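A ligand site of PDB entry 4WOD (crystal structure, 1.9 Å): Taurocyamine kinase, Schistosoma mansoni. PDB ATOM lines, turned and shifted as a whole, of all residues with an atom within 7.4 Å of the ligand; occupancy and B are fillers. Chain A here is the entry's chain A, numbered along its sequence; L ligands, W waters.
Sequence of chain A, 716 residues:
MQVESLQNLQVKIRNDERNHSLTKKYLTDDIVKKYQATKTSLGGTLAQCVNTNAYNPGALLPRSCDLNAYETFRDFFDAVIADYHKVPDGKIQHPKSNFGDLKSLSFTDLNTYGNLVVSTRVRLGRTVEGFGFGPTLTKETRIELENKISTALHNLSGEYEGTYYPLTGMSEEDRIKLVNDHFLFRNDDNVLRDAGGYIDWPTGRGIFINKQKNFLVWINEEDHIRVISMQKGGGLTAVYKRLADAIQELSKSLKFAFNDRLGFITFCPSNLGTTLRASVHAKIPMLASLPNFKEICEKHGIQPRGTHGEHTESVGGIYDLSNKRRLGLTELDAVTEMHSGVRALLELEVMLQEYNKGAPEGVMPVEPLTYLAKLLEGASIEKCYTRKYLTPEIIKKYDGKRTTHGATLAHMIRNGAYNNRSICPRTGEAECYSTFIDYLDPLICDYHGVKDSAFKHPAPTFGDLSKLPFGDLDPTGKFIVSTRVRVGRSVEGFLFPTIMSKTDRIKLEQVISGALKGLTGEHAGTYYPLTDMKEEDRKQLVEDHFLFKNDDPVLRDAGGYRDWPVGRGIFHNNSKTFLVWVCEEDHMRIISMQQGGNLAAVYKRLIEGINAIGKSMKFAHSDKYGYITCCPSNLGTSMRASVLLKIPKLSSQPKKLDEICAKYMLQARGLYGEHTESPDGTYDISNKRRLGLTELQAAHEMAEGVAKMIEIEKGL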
ATOM      1  N   SER A  21      32.549  19.138  -9.701  1.00  0.00           N
ATOM      2  CA  SER A  21      32.578  20.531 -10.162  1.00  0.00           C
ATOM      3  C   SER A  21      33.893  21.204  -9.805  1.00  0.00           C
ATOM      4  O   SER A  21      34.601  20.735  -8.923  1.00  0.00           O
ATOM      5  CB  SER A  21      31.404  21.309  -9.549  1.00  0.00           C
ATOM      6  OG  SER A  21      31.338  21.161  -8.125  1.00  0.00           O
ATOM      7  N   THR A  52      23.786  26.428  -5.919  1.00  0.00           N
ATOM      8  CA  THR A  52      23.287  25.574  -6.999  1.00  0.00           C
ATOM      9  C   THR A  52      24.166  24.318  -7.171  1.00  0.00           C
ATOM     10  O   THR A  52      23.669  23.269  -7.605  1.00  0.00           O
ATOM     11  CB  THR A  52      23.196  26.355  -8.343  1.00  0.00           C
ATOM     12  OG1 THR A  52      22.270  25.707  -9.224  1.00  0.00           O
ATOM     13  CG2 THR A  52      24.580  26.467  -9.005  1.00  0.00           C
ATOM     14  N   ASN A  53      25.440  24.391  -6.803  1.00  0.00           N
ATOM     15  CA  ASN A  53      26.307  23.224  -6.930  1.00  0.00           C
ATOM     16  C   ASN A  53      25.919  22.119  -5.964  1.00  0.00           C
ATOM     17  O   ASN A  53      26.098  20.936  -6.243  1.00  0.00           O
ATOM     18  CB  ASN A  53      27.760  23.589  -6.728  1.00  0.00           C
ATOM     19  CG  ASN A  53      28.267  24.532  -7.789  1.00  0.00           C
ATOM     20  OD1 ASN A  53      28.641  25.671  -7.482  1.00  0.00           O
ATOM     21  ND2 ASN A  53      28.297  24.073  -9.033  1.00  0.00           N
ATOM     22  N   GLY A  58      25.738  17.974 -11.669  1.00  0.00           N
ATOM     23  CA  GLY A  58      26.227  18.047 -13.040  1.00  0.00           C
ATOM     24  C   GLY A  58      26.819  19.398 -13.380  1.00  0.00           C
ATOM     25  O   GLY A  58      27.554  19.534 -14.349  1.00  0.00           O
ATOM     26  N   ALA A  59      26.504  20.406 -12.570  1.00  0.00           N
ATOM     27  CA  ALA A  59      26.994  21.762 -12.828  1.00  0.00           C
ATOM     28  C   ALA A  59      28.499  21.859 -12.541  1.00  0.00           C
ATOM     29  O   ALA A  59      28.967  21.474 -11.484  1.00  0.00           O
ATOM     30  CB  ALA A  59      26.226  22.761 -11.975  1.00  0.00           C
ATOM     31  N   LEU A  60      29.224  22.410 -13.504  1.00  0.00           N
ATOM     32  CA  LEU A  60      30.678  22.546 -13.408  1.00  0.00           C
ATOM     33  C   LEU A  60      31.149  23.770 -12.594  1.00  0.00           C
ATOM     34  O   LEU A  60      32.188  23.720 -11.929  1.00  0.00           O
ATOM     35  CB  LEU A  60      31.244  22.640 -14.825  1.00  0.00           C
ATOM     36  CG  LEU A  60      32.757  22.531 -14.940  1.00  0.00           C
ATOM     37  CD1 LEU A  60      33.187  21.171 -14.408  1.00  0.00           C
ATOM     38  CD2 LEU A  60      33.177  22.702 -16.401  1.00  0.00           C
ATOM     39  N   LEU A  61      30.385  24.842 -12.673  1.00  0.00           N
ATOM     40  CA  LEU A  61      30.797  26.154 -12.161  1.00  0.00           C
ATOM     41  C   LEU A  61      29.873  26.694 -11.063  1.00  0.00           C
ATOM     42  O   LEU A  61      28.713  26.320 -10.985  1.00  0.00           O
ATOM     43  CB  LEU A  61      30.847  27.159 -13.313  1.00  0.00           C
ATOM     44  CG  LEU A  61      31.911  26.883 -14.366  1.00  0.00           C
ATOM     45  CD1 LEU A  61      31.840  27.900 -15.491  1.00  0.00           C
ATOM     46  CD2 LEU A  61      33.297  26.873 -13.737  1.00  0.00           C
ATOM     47  N   PRO A  62      30.400  27.570 -10.187  1.00  0.00           N
ATOM     48  CA  PRO A  62      29.490  28.302  -9.295  1.00  0.00           C
ATOM     49  C   PRO A  62      28.738  29.352 -10.111  1.00  0.00           C
ATOM     50  O   PRO A  62      28.922  29.445 -11.329  1.00  0.00           O
ATOM     51  CB  PRO A  62      30.421  28.975  -8.285  1.00  0.00           C
ATOM     52  CG  PRO A  62      31.757  29.145  -9.074  1.00  0.00           C
ATOM     53  CD  PRO A  62      31.822  27.890  -9.937  1.00  0.00           C
ATOM     54  N   ARG A  63      27.931  30.170  -9.441  1.00  0.00           N
ATOM     55  CA  ARG A  63      27.458  31.377 -10.099  1.00  0.00           C
ATOM     56  C   ARG A  63      27.885  32.543  -9.224  1.00  0.00           C
ATOM     57  O   ARG A  63      28.755  32.387  -8.373  1.00  0.00           O
ATOM     58  CB  ARG A  63      25.942  31.324 -10.328  1.00  0.00           C
ATOM     59  CG  ARG A  63      25.486  30.120 -11.205  1.00  0.00           C
ATOM     60  CD  ARG A  63      25.968  30.250 -12.694  1.00  0.00           C
ATOM     61  NE  ARG A  63      25.454  29.198 -13.589  1.00  0.00           N
ATOM     62  CZ  ARG A  63      25.996  27.994 -13.743  1.00  0.00           C
ATOM     63  NH1 ARG A  63      27.088  27.634 -13.065  1.00  0.00           N
ATOM     64  NH2 ARG A  63      25.451  27.129 -14.597  1.00  0.00           N
ATOM     65  N   TYR A  84      38.900  26.889 -15.457  1.00  0.00           N
ATOM     66  CA  TYR A  84      37.922  26.737 -16.537  1.00  0.00           C
ATOM     67  C   TYR A  84      38.384  27.336 -17.864  1.00  0.00           C
ATOM     68  O   TYR A  84      38.210  26.743 -18.931  1.00  0.00           O
ATOM     69  CB  TYR A  84      36.576  27.379 -16.149  1.00  0.00           C
ATOM     70  CG  TYR A  84      35.513  27.166 -17.212  1.00  0.00           C
ATOM     71  CD1 TYR A  84      34.796  25.972 -17.278  1.00  0.00           C
ATOM     72  CD2 TYR A  84      35.238  28.149 -18.142  1.00  0.00           C
ATOM     73  CE1 TYR A  84      33.830  25.785 -18.261  1.00  0.00           C
ATOM     74  CE2 TYR A  84      34.291  27.957 -19.110  1.00  0.00           C
ATOM     75  CZ  TYR A  84      33.589  26.782 -19.169  1.00  0.00           C
ATOM     76  OH  TYR A  84      32.647  26.610 -20.143  1.00  0.00           O
ATOM     77  N   ARG A 123      26.046  35.955 -29.959  1.00  0.00           N
ATOM     78  CA  ARG A 123      25.446  36.301 -28.677  1.00  0.00           C
ATOM     79  C   ARG A 123      26.473  36.985 -27.778  1.00  0.00           C
ATOM     80  O   ARG A 123      27.648  36.607 -27.772  1.00  0.00           O
ATOM     81  CB  ARG A 123      24.912  35.035 -27.986  1.00  0.00           C
ATOM     82  CG  ARG A 123      24.406  35.254 -26.565  1.00  0.00           C
ATOM     83  CD  ARG A 123      24.804  34.091 -25.645  1.00  0.00           C
ATOM     84  NE  ARG A 123      26.128  34.306 -25.060  1.00  0.00           N
ATOM     85  CZ  ARG A 123      26.890  33.330 -24.575  1.00  0.00           C
ATOM     86  NH1 ARG A 123      26.475  32.069 -24.611  1.00  0.00           N
ATOM     87  NH2 ARG A 123      28.087  33.619 -24.061  1.00  0.00           N
ATOM     88  N   ASP A 189      15.310  25.708 -16.128  1.00  0.00           N
ATOM     89  CA  ASP A 189      16.688  25.283 -15.858  1.00  0.00           C
ATOM     90  C   ASP A 189      16.914  25.205 -14.349  1.00  0.00           C
ATOM     91  O   ASP A 189      16.923  26.233 -13.676  1.00  0.00           O
ATOM     92  CB  ASP A 189      17.671  26.267 -16.514  1.00  0.00           C
ATOM     93  CG  ASP A 189      19.158  25.864 -16.341  1.00  0.00           C
ATOM     94  OD1 ASP A 189      19.545  25.202 -15.357  1.00  0.00           O
ATOM     95  OD2 ASP A 189      19.962  26.264 -17.209  1.00  0.00           O
ATOM     96  N   VAL A 191      19.526  24.487 -12.626  1.00  0.00           N
ATOM     97  CA  VAL A 191      20.789  25.067 -12.159  1.00  0.00           C
ATOM     98  C   VAL A 191      20.525  26.554 -11.950  1.00  0.00           C
ATOM     99  O   VAL A 191      20.835  27.110 -10.889  1.00  0.00           O
ATOM    100  CB  VAL A 191      21.956  24.839 -13.167  1.00  0.00           C
ATOM    101  CG1 VAL A 191      23.173  25.671 -12.771  1.00  0.00           C
ATOM    102  CG2 VAL A 191      22.315  23.371 -13.261  1.00  0.00           C
ATOM    103  N   LEU A 192      19.915  27.179 -12.938  1.00  0.00           N
ATOM    104  CA  LEU A 192      19.542  28.586 -12.839  1.00  0.00           C
ATOM    105  C   LEU A 192      18.588  28.811 -11.665  1.00  0.00           C
ATOM    106  O   LEU A 192      18.744  29.767 -10.913  1.00  0.00           O
ATOM    107  CB  LEU A 192      18.915  29.079 -14.129  1.00  0.00           C
ATOM    108  CG  LEU A 192      18.636  30.580 -14.230  1.00  0.00           C
ATOM    109  CD1 LEU A 192      19.819  31.401 -13.722  1.00  0.00           C
ATOM    110  CD2 LEU A 192      18.282  30.960 -15.675  1.00  0.00           C
ATOM    111  N   GLU A 221      16.923  37.413 -17.778  1.00  0.00           N
ATOM    112  CA  GLU A 221      16.755  35.967 -17.872  1.00  0.00           C
ATOM    113  C   GLU A 221      17.788  35.259 -16.986  1.00  0.00           C
ATOM    114  O   GLU A 221      17.494  34.239 -16.362  1.00  0.00           O
ATOM    115  CB  GLU A 221      16.887  35.493 -19.327  1.00  0.00           C
ATOM    116  CG  GLU A 221      16.766  33.981 -19.493  1.00  0.00           C
ATOM    117  CD  GLU A 221      18.101  33.263 -19.494  1.00  0.00           C
ATOM    118  OE1 GLU A 221      19.113  33.877 -19.900  1.00  0.00           O
ATOM    119  OE2 GLU A 221      18.142  32.081 -19.104  1.00  0.00           O
ATOM    120  N   GLU A 222      18.988  35.815 -16.909  1.00  0.00           N
ATOM    121  CA  GLU A 222      20.086  35.255 -16.131  1.00  0.00           C
ATOM    122  C   GLU A 222      21.101  36.369 -15.913  1.00  0.00           C
ATOM    123  O   GLU A 222      21.343  36.808 -14.786  1.00  0.00           O
ATOM    124  CB  GLU A 222      20.738  34.067 -16.842  1.00  0.00           C
ATOM    125  CG  GLU A 222      22.097  33.702 -16.281  1.00  0.00           C
ATOM    126  CD  GLU A 222      22.702  32.441 -16.888  1.00  0.00           C
ATOM    127  OE1 GLU A 222      23.893  32.485 -17.258  1.00  0.00           O
ATOM    128  OE2 GLU A 222      21.999  31.405 -16.965  1.00  0.00           O
ATOM    129  N   ASP A 223      21.673  36.822 -17.031  1.00  0.00           N
ATOM    130  CA  ASP A 223      22.366  38.089 -17.054  1.00  0.00           C
ATOM    131  C   ASP A 223      21.368  39.214 -17.163  1.00  0.00           C
ATOM    132  O   ASP A 223      20.194  38.993 -17.484  1.00  0.00           O
ATOM    133  CB  ASP A 223      23.379  38.132 -18.212  1.00  0.00           C
ATOM    134  CG  ASP A 223      24.610  37.276 -17.928  1.00  0.00           C
ATOM    135  OD1 ASP A 223      25.227  37.465 -16.852  1.00  0.00           O
ATOM    136  OD2 ASP A 223      24.941  36.388 -18.742  1.00  0.00           O
ATOM    137  N   ARG A 226      21.035  39.913 -22.320  1.00  0.00           N
ATOM    138  CA  ARG A 226      21.630  39.006 -23.278  1.00  0.00           C
ATOM    139  C   ARG A 226      21.181  39.470 -24.658  1.00  0.00           C
ATOM    140  O   ARG A 226      19.978  39.581 -24.920  1.00  0.00           O
ATOM    141  CB  ARG A 226      21.247  37.533 -23.030  1.00  0.00           C
ATOM    142  CG  ARG A 226      22.132  36.601 -23.857  1.00  0.00           C
ATOM    143  CD  ARG A 226      22.064  35.118 -23.470  1.00  0.00           C
ATOM    144  NE  ARG A 226      22.384  34.769 -22.075  1.00  0.00           N
ATOM    145  CZ  ARG A 226      23.466  35.143 -21.383  1.00  0.00           C
ATOM    146  NH1 ARG A 226      23.606  34.716 -20.141  1.00  0.00           N
ATOM    147  NH2 ARG A 226      24.399  35.952 -21.897  1.00  0.00           N
ATOM    148  N   THR A 266      29.803  38.630 -15.858  1.00  0.00           N
ATOM    149  CA  THR A 266      28.568  37.908 -16.146  1.00  0.00           C
ATOM    150  C   THR A 266      28.189  37.083 -14.930  1.00  0.00           C
ATOM    151  O   THR A 266      29.027  36.875 -14.054  1.00  0.00           O
ATOM    152  CB  THR A 266      28.710  36.981 -17.366  1.00  0.00           C
ATOM    153  OG1 THR A 266      29.917  36.199 -17.230  1.00  0.00           O
ATOM    154  CG2 THR A 266      28.760  37.845 -18.649  1.00  0.00           C
ATOM    155  N   PHE A 267      26.947  36.612 -14.899  1.00  0.00           N
ATOM    156  CA  PHE A 267      26.435  35.784 -13.792  1.00  0.00           C
ATOM    157  C   PHE A 267      27.182  34.455 -13.692  1.00  0.00           C
ATOM    158  O   PHE A 267      27.531  33.993 -12.597  1.00  0.00           O
ATOM    159  CB  PHE A 267      24.928  35.547 -13.977  1.00  0.00           C
ATOM    160  CG  PHE A 267      24.279  34.700 -12.908  1.00  0.00           C
ATOM    161  CD1 PHE A 267      24.171  35.138 -11.602  1.00  0.00           C
ATOM    162  CD2 PHE A 267      23.729  33.464 -13.242  1.00  0.00           C
ATOM    163  CE1 PHE A 267      23.547  34.354 -10.636  1.00  0.00           C
ATOM    164  CE2 PHE A 267      23.097  32.689 -12.284  1.00  0.00           C
ATOM    165  CZ  PHE A 267      23.012  33.137 -10.977  1.00  0.00           C
ATOM    166  N   CYS A 268      27.432  33.834 -14.831  1.00  0.00           N
ATOM    167  CA  CYS A 268      28.198  32.584 -14.849  1.00  0.00           C
ATOM    168  C   CYS A 268      29.607  32.865 -15.315  1.00  0.00           C
ATOM    169  O   CYS A 268      29.803  33.614 -16.288  1.00  0.00           O
ATOM    170  CB  CYS A 268      27.525  31.553 -15.746  1.00  0.00           C
ATOM    171  SG  CYS A 268      28.431  30.007 -15.890  1.00  0.00           S
ATOM    172  N   PRO A 269      30.611  32.292 -14.617  1.00  0.00           N
ATOM    173  CA  PRO A 269      32.017  32.519 -14.964  1.00  0.00           C
ATOM    174  C   PRO A 269      32.417  32.054 -16.358  1.00  0.00           C
ATOM    175  O   PRO A 269      33.431  32.540 -16.852  1.00  0.00           O
ATOM    176  CB  PRO A 269      32.778  31.698 -13.908  1.00  0.00           C
ATOM    177  CG  PRO A 269      31.851  31.678 -12.720  1.00  0.00           C
ATOM    178  CD  PRO A 269      30.452  31.582 -13.331  1.00  0.00           C
ATOM    179  N   SER A 270      31.658  31.157 -16.976  1.00  0.00           N
ATOM    180  CA  SER A 270      32.036  30.644 -18.294  1.00  0.00           C
ATOM    181  C   SER A 270      31.956  31.712 -19.396  1.00  0.00           C
ATOM    182  O   SER A 270      32.638  31.608 -20.422  1.00  0.00           O
ATOM    183  CB  SER A 270      31.157  29.446 -18.682  1.00  0.00           C
ATOM    184  OG  SER A 270      29.799  29.827 -18.832  1.00  0.00           O
ATOM    185  N   ASN A 271      31.136  32.729 -19.166  1.00  0.00           N
ATOM    186  CA  ASN A 271      30.889  33.787 -20.158  1.00  0.00           C
ATOM    187  C   ASN A 271      31.555  35.130 -19.861  1.00  0.00           C
ATOM    188  O   ASN A 271      31.082  36.157 -20.340  1.00  0.00           O
ATOM    189  CB  ASN A 271      29.394  34.017 -20.308  1.00  0.00           C
ATOM    190  CG  ASN A 271      28.704  32.913 -21.079  1.00  0.00           C
ATOM    191  OD1 ASN A 271      29.184  32.500 -22.138  1.00  0.00           O
ATOM    192  ND2 ASN A 271      27.596  32.426 -20.551  1.00  0.00           N
ATOM    193  N   ARG A 305      28.419  21.581 -29.947  1.00  0.00           N
ATOM    194  CA  ARG A 305      27.323  21.153 -29.106  1.00  0.00           C
ATOM    195  C   ARG A 305      26.266  20.474 -29.948  1.00  0.00           C
ATOM    196  O   ARG A 305      25.902  20.960 -31.036  1.00  0.00           O
ATOM    197  CB  ARG A 305      26.720  22.335 -28.330  1.00  0.00           C
ATOM    198  CG  ARG A 305      27.650  22.963 -27.293  1.00  0.00           C
ATOM    199  CD  ARG A 305      27.323  24.442 -27.064  1.00  0.00           C
ATOM    200  NE  ARG A 305      28.075  25.051 -25.960  1.00  0.00           N
ATOM    201  CZ  ARG A 305      28.850  26.129 -26.100  1.00  0.00           C
ATOM    202  NH1 ARG A 305      28.994  26.687 -27.299  1.00  0.00           N
ATOM    203  NH2 ARG A 305      29.506  26.630 -25.057  1.00  0.00           N
HETATM  204  N1  LIG L   1      29.933  25.433 -17.473  1.00  0.00           N
HETATM  205  C1  LIG L   1      28.763  25.777 -16.709  1.00  0.00           C
HETATM  206  C2  LIG L   1      28.337  24.829 -15.604  1.00  0.00           C
HETATM  207  O1  LIG L   1      28.238  23.597 -15.826  1.00  0.00           O
HETATM  208  C3  LIG L   1      27.623  26.097 -17.602  1.00  0.00           C
HETATM  209  C4  LIG L   1      27.684  27.499 -18.119  1.00  0.00           C
HETATM  210  C5  LIG L   1      26.550  28.225 -17.492  1.00  0.00           C
HETATM  211  N2  LIG L   1      26.519  29.580 -17.948  1.00  0.00           N
HETATM  212  C6  LIG L   1      25.443  30.161 -18.393  1.00  0.00           C
HETATM  213  N3  LIG L   1      25.486  31.396 -18.780  1.00  0.00           N
HETATM  214  N4  LIG L   1      24.329  29.484 -18.457  1.00  0.00           N
HETATM  215  O2  LIG L   1      28.173  25.462 -14.548  1.00  0.00           O
HETATM  216  O   HOH W   1      24.994  24.435 -15.984  1.00  0.00           O
HETATM  217  O   HOH W   2      26.239  34.225 -17.328  1.00  0.00           O
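The side-chain carboxylate of Glu 222 lies within salt-bridge range of a nitrogen (N3) of the ligand (2.5 Å).
N of Leu 60 is in hydrogen-bond range of O1 of the ligand, 2.8 Å away.
A nitrogen (N2) of the ligand lies within hydrogen-bond range of the side-chain sulfur of Cys 268, 2.8 Å away.
The guanidinium group of Arg 63 is in salt-bridge range of an oxygen (O2) of the ligand, 2.8 Å away.
The side-chain amide nitrogen (ND2) of Asn 271 lies close to a nitrogen (N3) of the ligand, 2.9 Å away.
The backbone NH of Leu 61 sits at hydrogen-bond distance from an oxygen (O2) of the ligand (3.0 Å).
A nitrogen (N2) of the ligand lies close to the side-chain hydroxyl (OG) of Ser 270 (3.4 Å).
Merely in contact with the ligand: Ala 59 (3.7 Å) and Tyr 84 (3.98 Å).
Of the 25 residues printed, 9 come within 4 Å of the ligand.
The nearest printed residue that does not touch the ligand is Arg 226 (4.1 Å).
Water W1 bridges the guanidinium group of Arg 63 and an oxygen (O1) of the ligand.
The side-chain carboxylate of Glu 222 is in salt-bridge range of the guanidinium group of Arg 226 (3.7 Å).
SG of Cys 268 lies within hydrogen-bond range of OG of Ser 270 (3.2 Å).
O of Cys 268 sits at hydrogen-bond distance from OG1 of Thr 266 (2.8 Å).
The guanidinium group (NH1) of Arg 63 is in hydrogen-bond range of the backbone carbonyl oxygen (O) of Leu 61 (2.9 Å).
The guanidinium group of Arg 123 sits at hydrogen-bond distance from the side-chain amide oxygen of Asn 271.
O of Asn 271 sits close to OG1 of Thr 266.
ND2 of Asn 53 lies within hydrogen-bond range of O of Leu 61 (3.0 Å).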
